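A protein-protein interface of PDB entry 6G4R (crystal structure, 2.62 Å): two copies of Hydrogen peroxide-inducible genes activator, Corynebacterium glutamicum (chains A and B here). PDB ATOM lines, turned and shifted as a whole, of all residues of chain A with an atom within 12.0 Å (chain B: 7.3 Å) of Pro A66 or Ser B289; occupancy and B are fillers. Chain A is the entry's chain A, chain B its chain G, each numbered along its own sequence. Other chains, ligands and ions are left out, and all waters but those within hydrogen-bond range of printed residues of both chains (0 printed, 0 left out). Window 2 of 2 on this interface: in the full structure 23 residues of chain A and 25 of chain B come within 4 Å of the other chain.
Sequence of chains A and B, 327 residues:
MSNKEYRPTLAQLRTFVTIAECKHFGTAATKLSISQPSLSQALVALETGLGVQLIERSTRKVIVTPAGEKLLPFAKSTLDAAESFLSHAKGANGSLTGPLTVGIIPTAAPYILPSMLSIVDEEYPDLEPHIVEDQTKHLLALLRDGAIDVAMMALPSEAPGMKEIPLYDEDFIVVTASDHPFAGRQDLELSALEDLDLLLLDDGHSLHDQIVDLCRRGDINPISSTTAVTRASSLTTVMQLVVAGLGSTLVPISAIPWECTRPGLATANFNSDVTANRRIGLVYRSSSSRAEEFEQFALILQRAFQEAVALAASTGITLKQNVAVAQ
OG of Ser B289 touches O of Thr A65 (3.6 Å).
Ser B289 touches Pro A66 (O to CG, 3.4 Å).
Ala B92 touches Ala A67.
Ser B287 touches Glu A69 (O to OE2, 3.8 Å).
OE1 of Glu A69 touches CG of Arg B290 (3.3 Å).
Lys A70 touches Arg B290 (CD to NH2, 3.4 Å).
Lys A70 touches Glu B293 (CD to OE2, 3.8 Å).
Leu A71 touches Ala B92 (CD1 to CB, 3.97 Å).
The side-chain hydroxyl (OG1) of Thr A65 sits at hydrogen-bond distance from the backbone carbonyl oxygen (O) of Gln A53 (2.6 Å).
O of Leu A54 sits at hydrogen-bond distance from OG1 of Thr A65, 2.9 Å away.
N of Gly A68 lies within hydrogen-bond range of OG1 of Thr A65 (3.1 Å).
The backbone NH (N) of Arg B290 lies within hydrogen-bond range of the side-chain hydroxyl (OG) of Ser B288, at 3.2 Å.
The side-chain carboxylate (OE2) of Glu B293 lies within salt-bridge range of the guanidinium group (NH2) of Arg B290 (2.6 Å).
OG of Ser B289 sits at hydrogen-bond distance from O of Val A64, at 2.9 Å.
OG of Ser B288 sits at hydrogen-bond distance from OE1 of Glu A69 (3.2 Å).
N of Ser B289 lies within hydrogen-bond range of OE2 of Glu A69, 3.3 Å away.
The side-chain amino group (NZ) of Lys A70 is in hydrogen-bond range of the backbone carbonyl oxygen (O) of Ala B92 (2.7 Å).
No position is printed for both chains.
Ile A63 touches none of the printed residues of chain B.
Printed residues of chain B within 4 Å of Val A64: Ser B289.
Of the printed residues of chain B, Pro A66 touches Ser B289 (3.4 Å).
Printed residues of chain B within 4 Å of Ala A67: Ala B92.
Of the printed residues of chain A, Ser B287 touches Glu A69 (3.8 Å).
Of chain A, only Val A64, Thr A65, Pro A66 and Glu A69 come within 4 Å of Ser B289.
Of chain A, only Glu A69 (3.3 Å) and Lys A70 (3.4 Å) come within 4 Å of Arg B290.
Ala B291 touches none of the printed residues of chain A.
No residue of chain A comes within 4 Å of Glu B292.
The nearest residue of chain A that does not touch Ser B289 is Ile A63 (4.8 Å).
Of the 25 printed residues of chain A, 7 touch a printed residue of chain B.
Printed residues of chain A that touch a printed residue of chain B: Val A64, Thr A65, Pro A66, Ala A67, Glu A69, Lys A70 and Leu A71.
Of the 13 printed residues of chain B, 6 touch a printed residue of chain A.
Printed residues of chain B that touch a printed residue of chain A: Ala B92, Ser B287, Ser B288, Ser B289, Arg B290 and Glu B293.
Among the printed residues, no Asp or Glu carboxylate lies within 4 Å of a Lys or Arg side-chain nitrogen of the other chain.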
ATOM      1  N   PHE A  16      12.642  18.941  17.693  1.00  0.00           N
ATOM      2  CA  PHE A  16      12.791  19.520  19.023  1.00  0.00           C
ATOM      3  C   PHE A  16      11.665  20.499  19.333  1.00  0.00           C
ATOM      4  O   PHE A  16      11.173  20.551  20.467  1.00  0.00           O
ATOM      5  CB  PHE A  16      14.153  20.207  19.138  1.00  0.00           C
ATOM      6  CG  PHE A  16      14.294  21.072  20.356  1.00  0.00           C
ATOM      7  CD1 PHE A  16      14.239  20.519  21.623  1.00  0.00           C
ATOM      8  CD2 PHE A  16      14.483  22.439  20.232  1.00  0.00           C
ATOM      9  CE1 PHE A  16      14.367  21.312  22.746  1.00  0.00           C
ATOM     10  CE2 PHE A  16      14.612  23.238  21.353  1.00  0.00           C
ATOM     11  CZ  PHE A  16      14.553  22.673  22.611  1.00  0.00           C
ATOM     12  N   ILE A  19       8.231  18.485  19.786  1.00  0.00           N
ATOM     13  CA  ILE A  19       8.218  17.763  21.056  1.00  0.00           C
ATOM     14  C   ILE A  19       7.960  18.720  22.213  1.00  0.00           C
ATOM     15  O   ILE A  19       7.215  18.402  23.148  1.00  0.00           O
ATOM     16  CB  ILE A  19       9.531  16.978  21.246  1.00  0.00           C
ATOM     17  CG1 ILE A  19       9.608  15.821  20.248  1.00  0.00           C
ATOM     18  CG2 ILE A  19       9.650  16.457  22.669  1.00  0.00           C
ATOM     19  CD1 ILE A  19      10.909  15.053  20.307  1.00  0.00           C
ATOM     20  N   ALA A  20       8.578  19.902  22.180  1.00  0.00           N
ATOM     21  CA  ALA A  20       8.407  20.848  23.276  1.00  0.00           C
ATOM     22  C   ALA A  20       6.978  21.369  23.357  1.00  0.00           C
ATOM     23  O   ALA A  20       6.504  21.704  24.448  1.00  0.00           O
ATOM     24  CB  ALA A  20       9.387  22.011  23.123  1.00  0.00           C
ATOM     25  N   GLU A  21       6.277  21.448  22.225  1.00  0.00           N
ATOM     26  CA  GLU A  21       4.900  21.926  22.211  1.00  0.00           C
ATOM     27  C   GLU A  21       3.899  20.807  22.494  1.00  0.00           C
ATOM     28  O   GLU A  21       3.076  20.926  23.408  1.00  0.00           O
ATOM     29  CB  GLU A  21       4.597  22.603  20.870  1.00  0.00           C
ATOM     30  CG  GLU A  21       5.492  23.803  20.587  1.00  0.00           C
ATOM     31  CD  GLU A  21       5.104  24.548  19.325  1.00  0.00           C
ATOM     32  OE1 GLU A  21       4.034  24.245  18.757  1.00  0.00           O
ATOM     33  OE2 GLU A  21       5.871  25.439  18.902  1.00  0.00           O
ATOM     34  N   GLU A  47      20.870  16.223  20.341  1.00  0.00           N
ATOM     35  CA  GLU A  47      21.455  16.332  21.673  1.00  0.00           C
ATOM     36  C   GLU A  47      22.937  15.975  21.658  1.00  0.00           C
ATOM     37  O   GLU A  47      23.745  16.632  22.325  1.00  0.00           O
ATOM     38  CB  GLU A  47      20.698  15.440  22.658  1.00  0.00           C
ATOM     39  CG  GLU A  47      19.269  15.884  22.927  1.00  0.00           C
ATOM     40  N   GLY A  51      25.853  18.325  22.518  1.00  0.00           N
ATOM     41  CA  GLY A  51      26.390  17.936  23.808  1.00  0.00           C
ATOM     42  C   GLY A  51      25.647  18.502  24.997  1.00  0.00           C
ATOM     43  O   GLY A  51      26.267  18.793  26.024  1.00  0.00           O
ATOM     44  N   VAL A  52      24.329  18.663  24.887  1.00  0.00           N
ATOM     45  CA  VAL A  52      23.508  19.201  25.964  1.00  0.00           C
ATOM     46  C   VAL A  52      22.175  18.465  25.985  1.00  0.00           C
ATOM     47  O   VAL A  52      21.675  18.014  24.950  1.00  0.00           O
ATOM     48  CB  VAL A  52      23.292  20.725  25.821  1.00  0.00           C
ATOM     49  CG1 VAL A  52      24.518  21.485  26.294  1.00  0.00           C
ATOM     50  CG2 VAL A  52      22.990  21.078  24.377  1.00  0.00           C
ATOM     51  N   GLN A  53      21.602  18.347  27.180  1.00  0.00           N
ATOM     52  CA  GLN A  53      20.334  17.649  27.380  1.00  0.00           C
ATOM     53  C   GLN A  53      19.191  18.638  27.175  1.00  0.00           C
ATOM     54  O   GLN A  53      19.023  19.578  27.960  1.00  0.00           O
ATOM     55  CB  GLN A  53      20.280  17.023  28.771  1.00  0.00           C
ATOM     56  CG  GLN A  53      18.965  16.333  29.110  1.00  0.00           C
ATOM     57  CD  GLN A  53      18.849  14.942  28.514  1.00  0.00           C
ATOM     58  OE1 GLN A  53      19.682  14.523  27.709  1.00  0.00           O
ATOM     59  NE2 GLN A  53      17.813  14.212  28.914  1.00  0.00           N
ATOM     60  N   LEU A  54      18.404  18.424  26.121  1.00  0.00           N
ATOM     61  CA  LEU A  54      17.267  19.279  25.802  1.00  0.00           C
ATOM     62  C   LEU A  54      15.940  18.733  26.301  1.00  0.00           C
ATOM     63  O   LEU A  54      15.054  19.520  26.653  1.00  0.00           O
ATOM     64  CB  LEU A  54      17.165  19.507  24.287  1.00  0.00           C
ATOM     65  CG  LEU A  54      18.085  20.499  23.562  1.00  0.00           C
ATOM     66  CD1 LEU A  54      19.539  20.377  23.976  1.00  0.00           C
ATOM     67  CD2 LEU A  54      17.949  20.328  22.055  1.00  0.00           C
ATOM     68  N   ILE A  55      15.777  17.413  26.342  1.00  0.00           N
ATOM     69  CA  ILE A  55      14.512  16.784  26.698  1.00  0.00           C
ATOM     70  C   ILE A  55      14.769  15.782  27.814  1.00  0.00           C
ATOM     71  O   ILE A  55      15.717  14.992  27.739  1.00  0.00           O
ATOM     72  CB  ILE A  55      13.868  16.093  25.481  1.00  0.00           C
ATOM     73  CG1 ILE A  55      13.418  17.135  24.456  1.00  0.00           C
ATOM     74  CG2 ILE A  55      12.693  15.229  25.912  1.00  0.00           C
ATOM     75  CD1 ILE A  55      12.353  18.078  24.965  1.00  0.00           C
ATOM     76  N   GLU A  56      13.933  15.819  28.847  1.00  0.00           N
ATOM     77  CA  GLU A  56      14.029  14.867  29.948  1.00  0.00           C
ATOM     78  C   GLU A  56      13.013  13.741  29.786  1.00  0.00           C
ATOM     79  O   GLU A  56      12.646  13.378  28.668  1.00  0.00           O
ATOM     80  CB  GLU A  56      13.821  15.574  31.289  1.00  0.00           C
ATOM     81  N   LYS A  61       6.364  10.727  30.978  1.00  0.00           N
ATOM     82  CA  LYS A  61       5.949  12.014  30.440  1.00  0.00           C
ATOM     83  C   LYS A  61       7.170  12.906  30.278  1.00  0.00           C
ATOM     84  O   LYS A  61       8.050  12.931  31.143  1.00  0.00           O
ATOM     85  CB  LYS A  61       4.901  12.685  31.338  1.00  0.00           C
ATOM     86  CG  LYS A  61       5.031  12.342  32.814  1.00  0.00           C
ATOM     87  CD  LYS A  61       3.864  12.891  33.625  1.00  0.00           C
ATOM     88  CE  LYS A  61       4.165  14.272  34.197  1.00  0.00           C
ATOM     89  NZ  LYS A  61       4.401  15.304  33.149  1.00  0.00           N
ATOM     90  N   VAL A  62       7.215  13.635  29.167  1.00  0.00           N
ATOM     91  CA  VAL A  62       8.390  14.400  28.767  1.00  0.00           C
ATOM     92  C   VAL A  62       8.273  15.832  29.269  1.00  0.00           C
ATOM     93  O   VAL A  62       7.213  16.463  29.166  1.00  0.00           O
ATOM     94  CB  VAL A  62       8.569  14.352  27.236  1.00  0.00           C
ATOM     95  CG1 VAL A  62       9.157  15.655  26.711  1.00  0.00           C
ATOM     96  CG2 VAL A  62       9.450  13.175  26.846  1.00  0.00           C
ATOM     97  N   ILE A  63       9.370  16.344  29.826  1.00  0.00           N
ATOM     98  CA  ILE A  63       9.489  17.736  30.237  1.00  0.00           C
ATOM     99  C   ILE A  63      10.699  18.336  29.536  1.00  0.00           C
ATOM    100  O   ILE A  63      11.697  17.652  29.286  1.00  0.00           O
ATOM    101  CB  ILE A  63       9.620  17.886  31.769  1.00  0.00           C
ATOM    102  CG1 ILE A  63       8.687  16.912  32.491  1.00  0.00           C
ATOM    103  CG2 ILE A  63       9.322  19.317  32.197  1.00  0.00           C
ATOM    104  CD1 ILE A  63       8.766  16.999  33.999  1.00  0.00           C
ATOM    105  N   VAL A  64      10.608  19.624  29.215  1.00  0.00           N
ATOM    106  CA  VAL A  64      11.720  20.328  28.586  1.00  0.00           C
ATOM    107  C   VAL A  64      12.714  20.740  29.663  1.00  0.00           C
ATOM    108  O   VAL A  64      12.329  21.290  30.703  1.00  0.00           O
ATOM    109  CB  VAL A  64      11.217  21.545  27.793  1.00  0.00           C
ATOM    110  CG1 VAL A  64      12.372  22.222  27.069  1.00  0.00           C
ATOM    111  CG2 VAL A  64      10.135  21.127  26.809  1.00  0.00           C
ATOM    112  N   THR A  65      13.995  20.474  29.418  1.00  0.00           N
ATOM    113  CA  THR A  65      15.029  20.766  30.395  1.00  0.00           C
ATOM    114  C   THR A  65      15.239  22.274  30.518  1.00  0.00           C
ATOM    115  O   THR A  65      14.831  23.039  29.640  1.00  0.00           O
ATOM    116  CB  THR A  65      16.338  20.086  29.999  1.00  0.00           C
ATOM    117  OG1 THR A  65      16.768  20.581  28.726  1.00  0.00           O
ATOM    118  CG2 THR A  65      16.147  18.579  29.914  1.00  0.00           C
ATOM    119  N   PRO A  66      15.853  22.727  31.619  1.00  0.00           N
ATOM    120  CA  PRO A  66      16.197  24.158  31.723  1.00  0.00           C
ATOM    121  C   PRO A  66      16.980  24.682  30.530  1.00  0.00           C
ATOM    122  O   PRO A  66      16.679  25.767  30.019  1.00  0.00           O
ATOM    123  CB  PRO A  66      17.012  24.217  33.021  1.00  0.00           C
ATOM    124  CG  PRO A  66      16.500  23.088  33.840  1.00  0.00           C
ATOM    125  CD  PRO A  66      16.078  22.005  32.884  1.00  0.00           C
ATOM    126  N   ALA A  67      17.988  23.933  30.072  1.00  0.00           N
ATOM    127  CA  ALA A  67      18.737  24.348  28.890  1.00  0.00           C
ATOM    128  C   ALA A  67      17.870  24.326  27.638  1.00  0.00           C
ATOM    129  O   ALA A  67      18.083  25.134  26.725  1.00  0.00           O
ATOM    130  CB  ALA A  67      19.962  23.454  28.704  1.00  0.00           C
ATOM    131  N   GLY A  68      16.901  23.413  27.569  1.00  0.00           N
ATOM    132  CA  GLY A  68      16.027  23.363  26.409  1.00  0.00           C
ATOM    133  C   GLY A  68      15.104  24.564  26.305  1.00  0.00           C
ATOM    134  O   GLY A  68      14.804  25.031  25.203  1.00  0.00           O
ATOM    135  N   GLU A  69      14.637  25.076  27.448  1.00  0.00           N
ATOM    136  CA  GLU A  69      13.741  26.229  27.426  1.00  0.00           C
ATOM    137  C   GLU A  69      14.439  27.469  26.880  1.00  0.00           C
ATOM    138  O   GLU A  69      13.821  28.278  26.179  1.00  0.00           O
ATOM    139  CB  GLU A  69      13.181  26.497  28.823  1.00  0.00           C
ATOM    140  CG  GLU A  69      11.989  25.625  29.182  1.00  0.00           C
ATOM    141  CD  GLU A  69      11.024  26.313  30.131  1.00  0.00           C
ATOM    142  OE1 GLU A  69      11.402  27.346  30.722  1.00  0.00           O
ATOM    143  OE2 GLU A  69       9.884  25.825  30.278  1.00  0.00           O
ATOM    144  N   LYS A  70      15.724  27.642  27.197  1.00  0.00           N
ATOM    145  CA  LYS A  70      16.446  28.808  26.698  1.00  0.00           C
ATOM    146  C   LYS A  70      16.681  28.721  25.196  1.00  0.00           C
ATOM    147  O   LYS A  70      16.737  29.753  24.518  1.00  0.00           O
ATOM    148  CB  LYS A  70      17.780  28.964  27.431  1.00  0.00           C
ATOM    149  CG  LYS A  70      17.665  29.012  28.947  1.00  0.00           C
ATOM    150  CD  LYS A  70      18.848  29.742  29.569  1.00  0.00           C
ATOM    151  CE  LYS A  70      20.176  29.134  29.142  1.00  0.00           C
ATOM    152  NZ  LYS A  70      20.291  27.702  29.532  1.00  0.00           N
ATOM    153  N   LEU A  71      16.819  27.507  24.661  1.00  0.00           N
ATOM    154  CA  LEU A  71      17.104  27.313  23.246  1.00  0.00           C
ATOM    155  C   LEU A  71      15.856  27.248  22.380  1.00  0.00           C
ATOM    156  O   LEU A  71      15.944  27.517  21.175  1.00  0.00           O
ATOM    157  CB  LEU A  71      17.918  26.031  23.047  1.00  0.00           C
ATOM    158  CG  LEU A  71      19.345  26.117  23.578  1.00  0.00           C
ATOM    159  CD1 LEU A  71      20.053  24.775  23.468  1.00  0.00           C
ATOM    160  CD2 LEU A  71      20.085  27.191  22.814  1.00  0.00           C
ATOM    161  N   LEU A  72      14.710  26.889  22.957  1.00  0.00           N
ATOM    162  CA  LEU A  72      13.480  26.716  22.186  1.00  0.00           C
ATOM    163  C   LEU A  72      13.094  27.944  21.364  1.00  0.00           C
ATOM    164  O   LEU A  72      12.736  27.775  20.187  1.00  0.00           O
ATOM    165  CB  LEU A  72      12.357  26.288  23.146  1.00  0.00           C
ATOM    166  CG  LEU A  72      10.965  25.919  22.616  1.00  0.00           C
ATOM    167  CD1 LEU A  72      10.065  27.139  22.474  1.00  0.00           C
ATOM    168  CD2 LEU A  72      11.063  25.156  21.299  1.00  0.00           C
ATOM    169  N   PRO A  73      13.125  29.177  21.891  1.00  0.00           N
ATOM    170  CA  PRO A  73      12.772  30.326  21.036  1.00  0.00           C
ATOM    171  C   PRO A  73      13.699  30.503  19.845  1.00  0.00           C
ATOM    172  O   PRO A  73      13.242  30.903  18.766  1.00  0.00           O
ATOM    173  CB  PRO A  73      12.852  31.518  22.000  1.00  0.00           C
ATOM    174  CG  PRO A  73      12.673  30.930  23.350  1.00  0.00           C
ATOM    175  CD  PRO A  73      13.344  29.596  23.288  1.00  0.00           C
ATOM    176  N   PHE A  74      14.993  30.217  20.007  1.00  0.00           N
ATOM    177  CA  PHE A  74      15.923  30.352  18.890  1.00  0.00           C
ATOM    178  C   PHE A  74      15.661  29.317  17.805  1.00  0.00           C
ATOM    179  O   PHE A  74      15.891  29.592  16.622  1.00  0.00           O
ATOM    180  CB  PHE A  74      17.365  30.245  19.386  1.00  0.00           C
ATOM    181  CG  PHE A  74      17.729  31.279  20.411  1.00  0.00           C
ATOM    182  CD1 PHE A  74      17.990  32.584  20.030  1.00  0.00           C
ATOM    183  CD2 PHE A  74      17.813  30.947  21.751  1.00  0.00           C
ATOM    184  CE1 PHE A  74      18.325  33.539  20.968  1.00  0.00           C
ATOM    185  CE2 PHE A  74      18.149  31.898  22.694  1.00  0.00           C
ATOM    186  CZ  PHE A  74      18.405  33.195  22.302  1.00  0.00           C
ATOM    187  N   ALA B  92      24.293  26.929  27.114  1.00  0.00           N
ATOM    188  CA  ALA B  92      23.017  26.394  27.584  1.00  0.00           C
ATOM    189  C   ALA B  92      23.147  25.725  28.948  1.00  0.00           C
ATOM    190  O   ALA B  92      22.265  25.877  29.803  1.00  0.00           O
ATOM    191  CB  ALA B  92      22.456  25.409  26.559  1.00  0.00           C
ATOM    192  N   GLY B  94      24.693  26.443  31.485  1.00  0.00           N
ATOM    193  CA  GLY B  94      25.026  27.339  32.568  1.00  0.00           C
ATOM    194  C   GLY B  94      23.793  27.898  33.260  1.00  0.00           C
ATOM    195  O   GLY B  94      22.669  27.793  32.778  1.00  0.00           O
ATOM    196  N   TYR B 284       6.827  34.222  37.682  1.00  0.00           N
ATOM    197  CA  TYR B 284       7.124  33.495  36.457  1.00  0.00           C
ATOM    198  C   TYR B 284       6.060  32.427  36.247  1.00  0.00           C
ATOM    199  O   TYR B 284       5.229  32.167  37.122  1.00  0.00           O
ATOM    200  CB  TYR B 284       8.529  32.876  36.496  1.00  0.00           C
ATOM    201  CG  TYR B 284       8.737  31.868  37.607  1.00  0.00           C
ATOM    202  CD1 TYR B 284       9.014  32.283  38.904  1.00  0.00           C
ATOM    203  CD2 TYR B 284       8.669  30.504  37.357  1.00  0.00           C
ATOM    204  CE1 TYR B 284       9.207  31.369  39.921  1.00  0.00           C
ATOM    205  CE2 TYR B 284       8.861  29.582  38.369  1.00  0.00           C
ATOM    206  CZ  TYR B 284       9.131  30.020  39.648  1.00  0.00           C
ATOM    207  OH  TYR B 284       9.325  29.107  40.660  1.00  0.00           O
ATOM    208  N   ARG B 285       6.087  31.809  35.068  1.00  0.00           N
ATOM    209  CA  ARG B 285       5.071  30.826  34.715  1.00  0.00           C
ATOM    210  C   ARG B 285       5.277  29.525  35.482  1.00  0.00           C
ATOM    211  O   ARG B 285       6.409  29.111  35.744  1.00  0.00           O
ATOM    212  CB  ARG B 285       5.095  30.554  33.211  1.00  0.00           C
ATOM    213  CG  ARG B 285       4.770  31.763  32.348  1.00  0.00           C
ATOM    214  CD  ARG B 285       4.847  31.420  30.868  1.00  0.00           C
ATOM    215  NE  ARG B 285       6.221  31.217  30.416  1.00  0.00           N
ATOM    216  CZ  ARG B 285       6.978  32.168  29.880  1.00  0.00           C
ATOM    217  NH1 ARG B 285       6.498  33.394  29.726  1.00  0.00           N
ATOM    218  NH2 ARG B 285       8.218  31.894  29.496  1.00  0.00           N
ATOM    219  N   SER B 286       4.165  28.879  35.839  1.00  0.00           N
ATOM    220  CA  SER B 286       4.245  27.598  36.536  1.00  0.00           C
ATOM    221  C   SER B 286       4.788  26.498  35.633  1.00  0.00           C
ATOM    222  O   SER B 286       5.497  25.603  36.107  1.00  0.00           O
ATOM    223  CB  SER B 286       2.870  27.210  37.079  1.00  0.00           C
ATOM    224  OG  SER B 286       2.558  27.943  38.250  1.00  0.00           O
ATOM    225  N   SER B 287       4.466  26.543  34.338  1.00  0.00           N
ATOM    226  CA  SER B 287       4.963  25.544  33.400  1.00  0.00           C
ATOM    227  C   SER B 287       6.465  25.640  33.176  1.00  0.00           C
ATOM    228  O   SER B 287       7.048  24.710  32.608  1.00  0.00           O
ATOM    229  CB  SER B 287       4.238  25.677  32.059  1.00  0.00           C
ATOM    230  OG  SER B 287       4.408  26.974  31.513  1.00  0.00           O
ATOM    231  N   SER B 288       7.097  26.732  33.597  1.00  0.00           N
ATOM    232  CA  SER B 288       8.521  26.918  33.365  1.00  0.00           C
ATOM    233  C   SER B 288       9.339  25.899  34.149  1.00  0.00           C
ATOM    234  O   SER B 288       9.008  25.550  35.285  1.00  0.00           O
ATOM    235  CB  SER B 288       8.941  28.335  33.756  1.00  0.00           C
ATOM    236  OG  SER B 288      10.317  28.549  33.504  1.00  0.00           O
ATOM    237  N   SER B 289      10.419  25.426  33.530  1.00  0.00           N
ATOM    238  CA  SER B 289      11.364  24.520  34.165  1.00  0.00           C
ATOM    239  C   SER B 289      12.632  25.240  34.599  1.00  0.00           C
ATOM    240  O   SER B 289      13.611  24.589  34.976  1.00  0.00           O
ATOM    241  CB  SER B 289      11.711  23.366  33.221  1.00  0.00           C
ATOM    242  OG  SER B 289      12.192  23.846  31.979  1.00  0.00           O
ATOM    243  N   ARG B 290      12.628  26.572  34.551  1.00  0.00           N
ATOM    244  CA  ARG B 290      13.772  27.399  34.910  1.00  0.00           C
ATOM    245  C   ARG B 290      13.631  27.985  36.311  1.00  0.00           C
ATOM    246  O   ARG B 290      14.095  29.102  36.566  1.00  0.00           O
ATOM    247  CB  ARG B 290      13.931  28.515  33.879  1.00  0.00           C
ATOM    248  CG  ARG B 290      14.171  28.013  32.462  1.00  0.00           C
ATOM    249  CD  ARG B 290      14.147  29.150  31.450  1.00  0.00           C
ATOM    250  NE  ARG B 290      15.325  30.008  31.519  1.00  0.00           N
ATOM    251  CZ  ARG B 290      15.490  31.100  30.779  1.00  0.00           C
ATOM    252  NH1 ARG B 290      14.550  31.464  29.917  1.00  0.00           N
ATOM    253  NH2 ARG B 290      16.590  31.829  30.900  1.00  0.00           N
ATOM    254  N   ALA B 291      12.982  27.250  37.218  1.00  0.00           N
ATOM    255  CA  ALA B 291      12.781  27.732  38.581  1.00  0.00           C
ATOM    256  C   ALA B 291      14.109  28.037  39.263  1.00  0.00           C
ATOM    257  O   ALA B 291      14.303  29.130  39.811  1.00  0.00           O
ATOM    258  CB  ALA B 291      11.983  26.706  39.387  1.00  0.00           C
ATOM    259  N   GLU B 292      15.043  27.083  39.232  1.00  0.00           N
ATOM    260  CA  GLU B 292      16.327  27.270  39.898  1.00  0.00           C
ATOM    261  C   GLU B 292      17.149  28.383  39.263  1.00  0.00           C
ATOM    262  O   GLU B 292      18.008  28.964  39.938  1.00  0.00           O
ATOM    263  CB  GLU B 292      17.110  25.957  39.896  1.00  0.00           C
ATOM    264  CG  GLU B 292      16.464  24.866  40.739  1.00  0.00           C
ATOM    265  CD  GLU B 292      17.290  23.596  40.795  1.00  0.00           C
ATOM    266  OE1 GLU B 292      16.940  22.693  41.584  1.00  0.00           O
ATOM    267  OE2 GLU B 292      18.290  23.502  40.053  1.00  0.00           O
ATOM    268  N   GLU B 293      16.914  28.683  37.985  1.00  0.00           N
ATOM    269  CA  GLU B 293      17.581  29.812  37.347  1.00  0.00           C
ATOM    270  C   GLU B 293      16.975  31.137  37.793  1.00  0.00           C
ATOM    271  O   GLU B 293      17.700  32.114  38.008  1.00  0.00           O
ATOM    272  CB  GLU B 293      17.502  29.671  35.826  1.00  0.00           C
ATOM    273  CG  GLU B 293      18.058  30.858  35.060  1.00  0.00           C
ATOM    274  CD  GLU B 293      17.972  30.679  33.556  1.00  0.00           C
ATOM    275  OE1 GLU B 293      17.509  29.610  33.108  1.00  0.00           O
ATOM    276  OE2 GLU B 293      18.366  31.611  32.824  1.00  0.00           O
ATOM    277  N   PHE B 294      15.650  31.183  37.943  1.00  0.00           N
ATOM    278  CA  PHE B 294      14.995  32.406  38.392  1.00  0.00           C
ATOM    279  C   PHE B 294      15.279  32.676  39.864  1.00  0.00           C
ATOM    280  O   PHE B 294      15.410  33.836  40.272  1.00  0.00           O
ATOM    281  CB  PHE B 294      13.486  32.318  38.154  1.00  0.00           C
ATOM    282  CG  PHE B 294      13.103  32.235  36.706  1.00  0.00           C
ATOM    283  CD1 PHE B 294      13.901  32.806  35.728  1.00  0.00           C
ATOM    284  CD2 PHE B 294      11.941  31.586  36.321  1.00  0.00           C
ATOM    285  CE1 PHE B 294      13.548  32.731  34.394  1.00  0.00           C
ATOM    286  CE2 PHE B 294      11.582  31.508  34.988  1.00  0.00           C
ATOM    287  CZ  PHE B 294      12.387  32.081  34.024  1.00  0.00           C
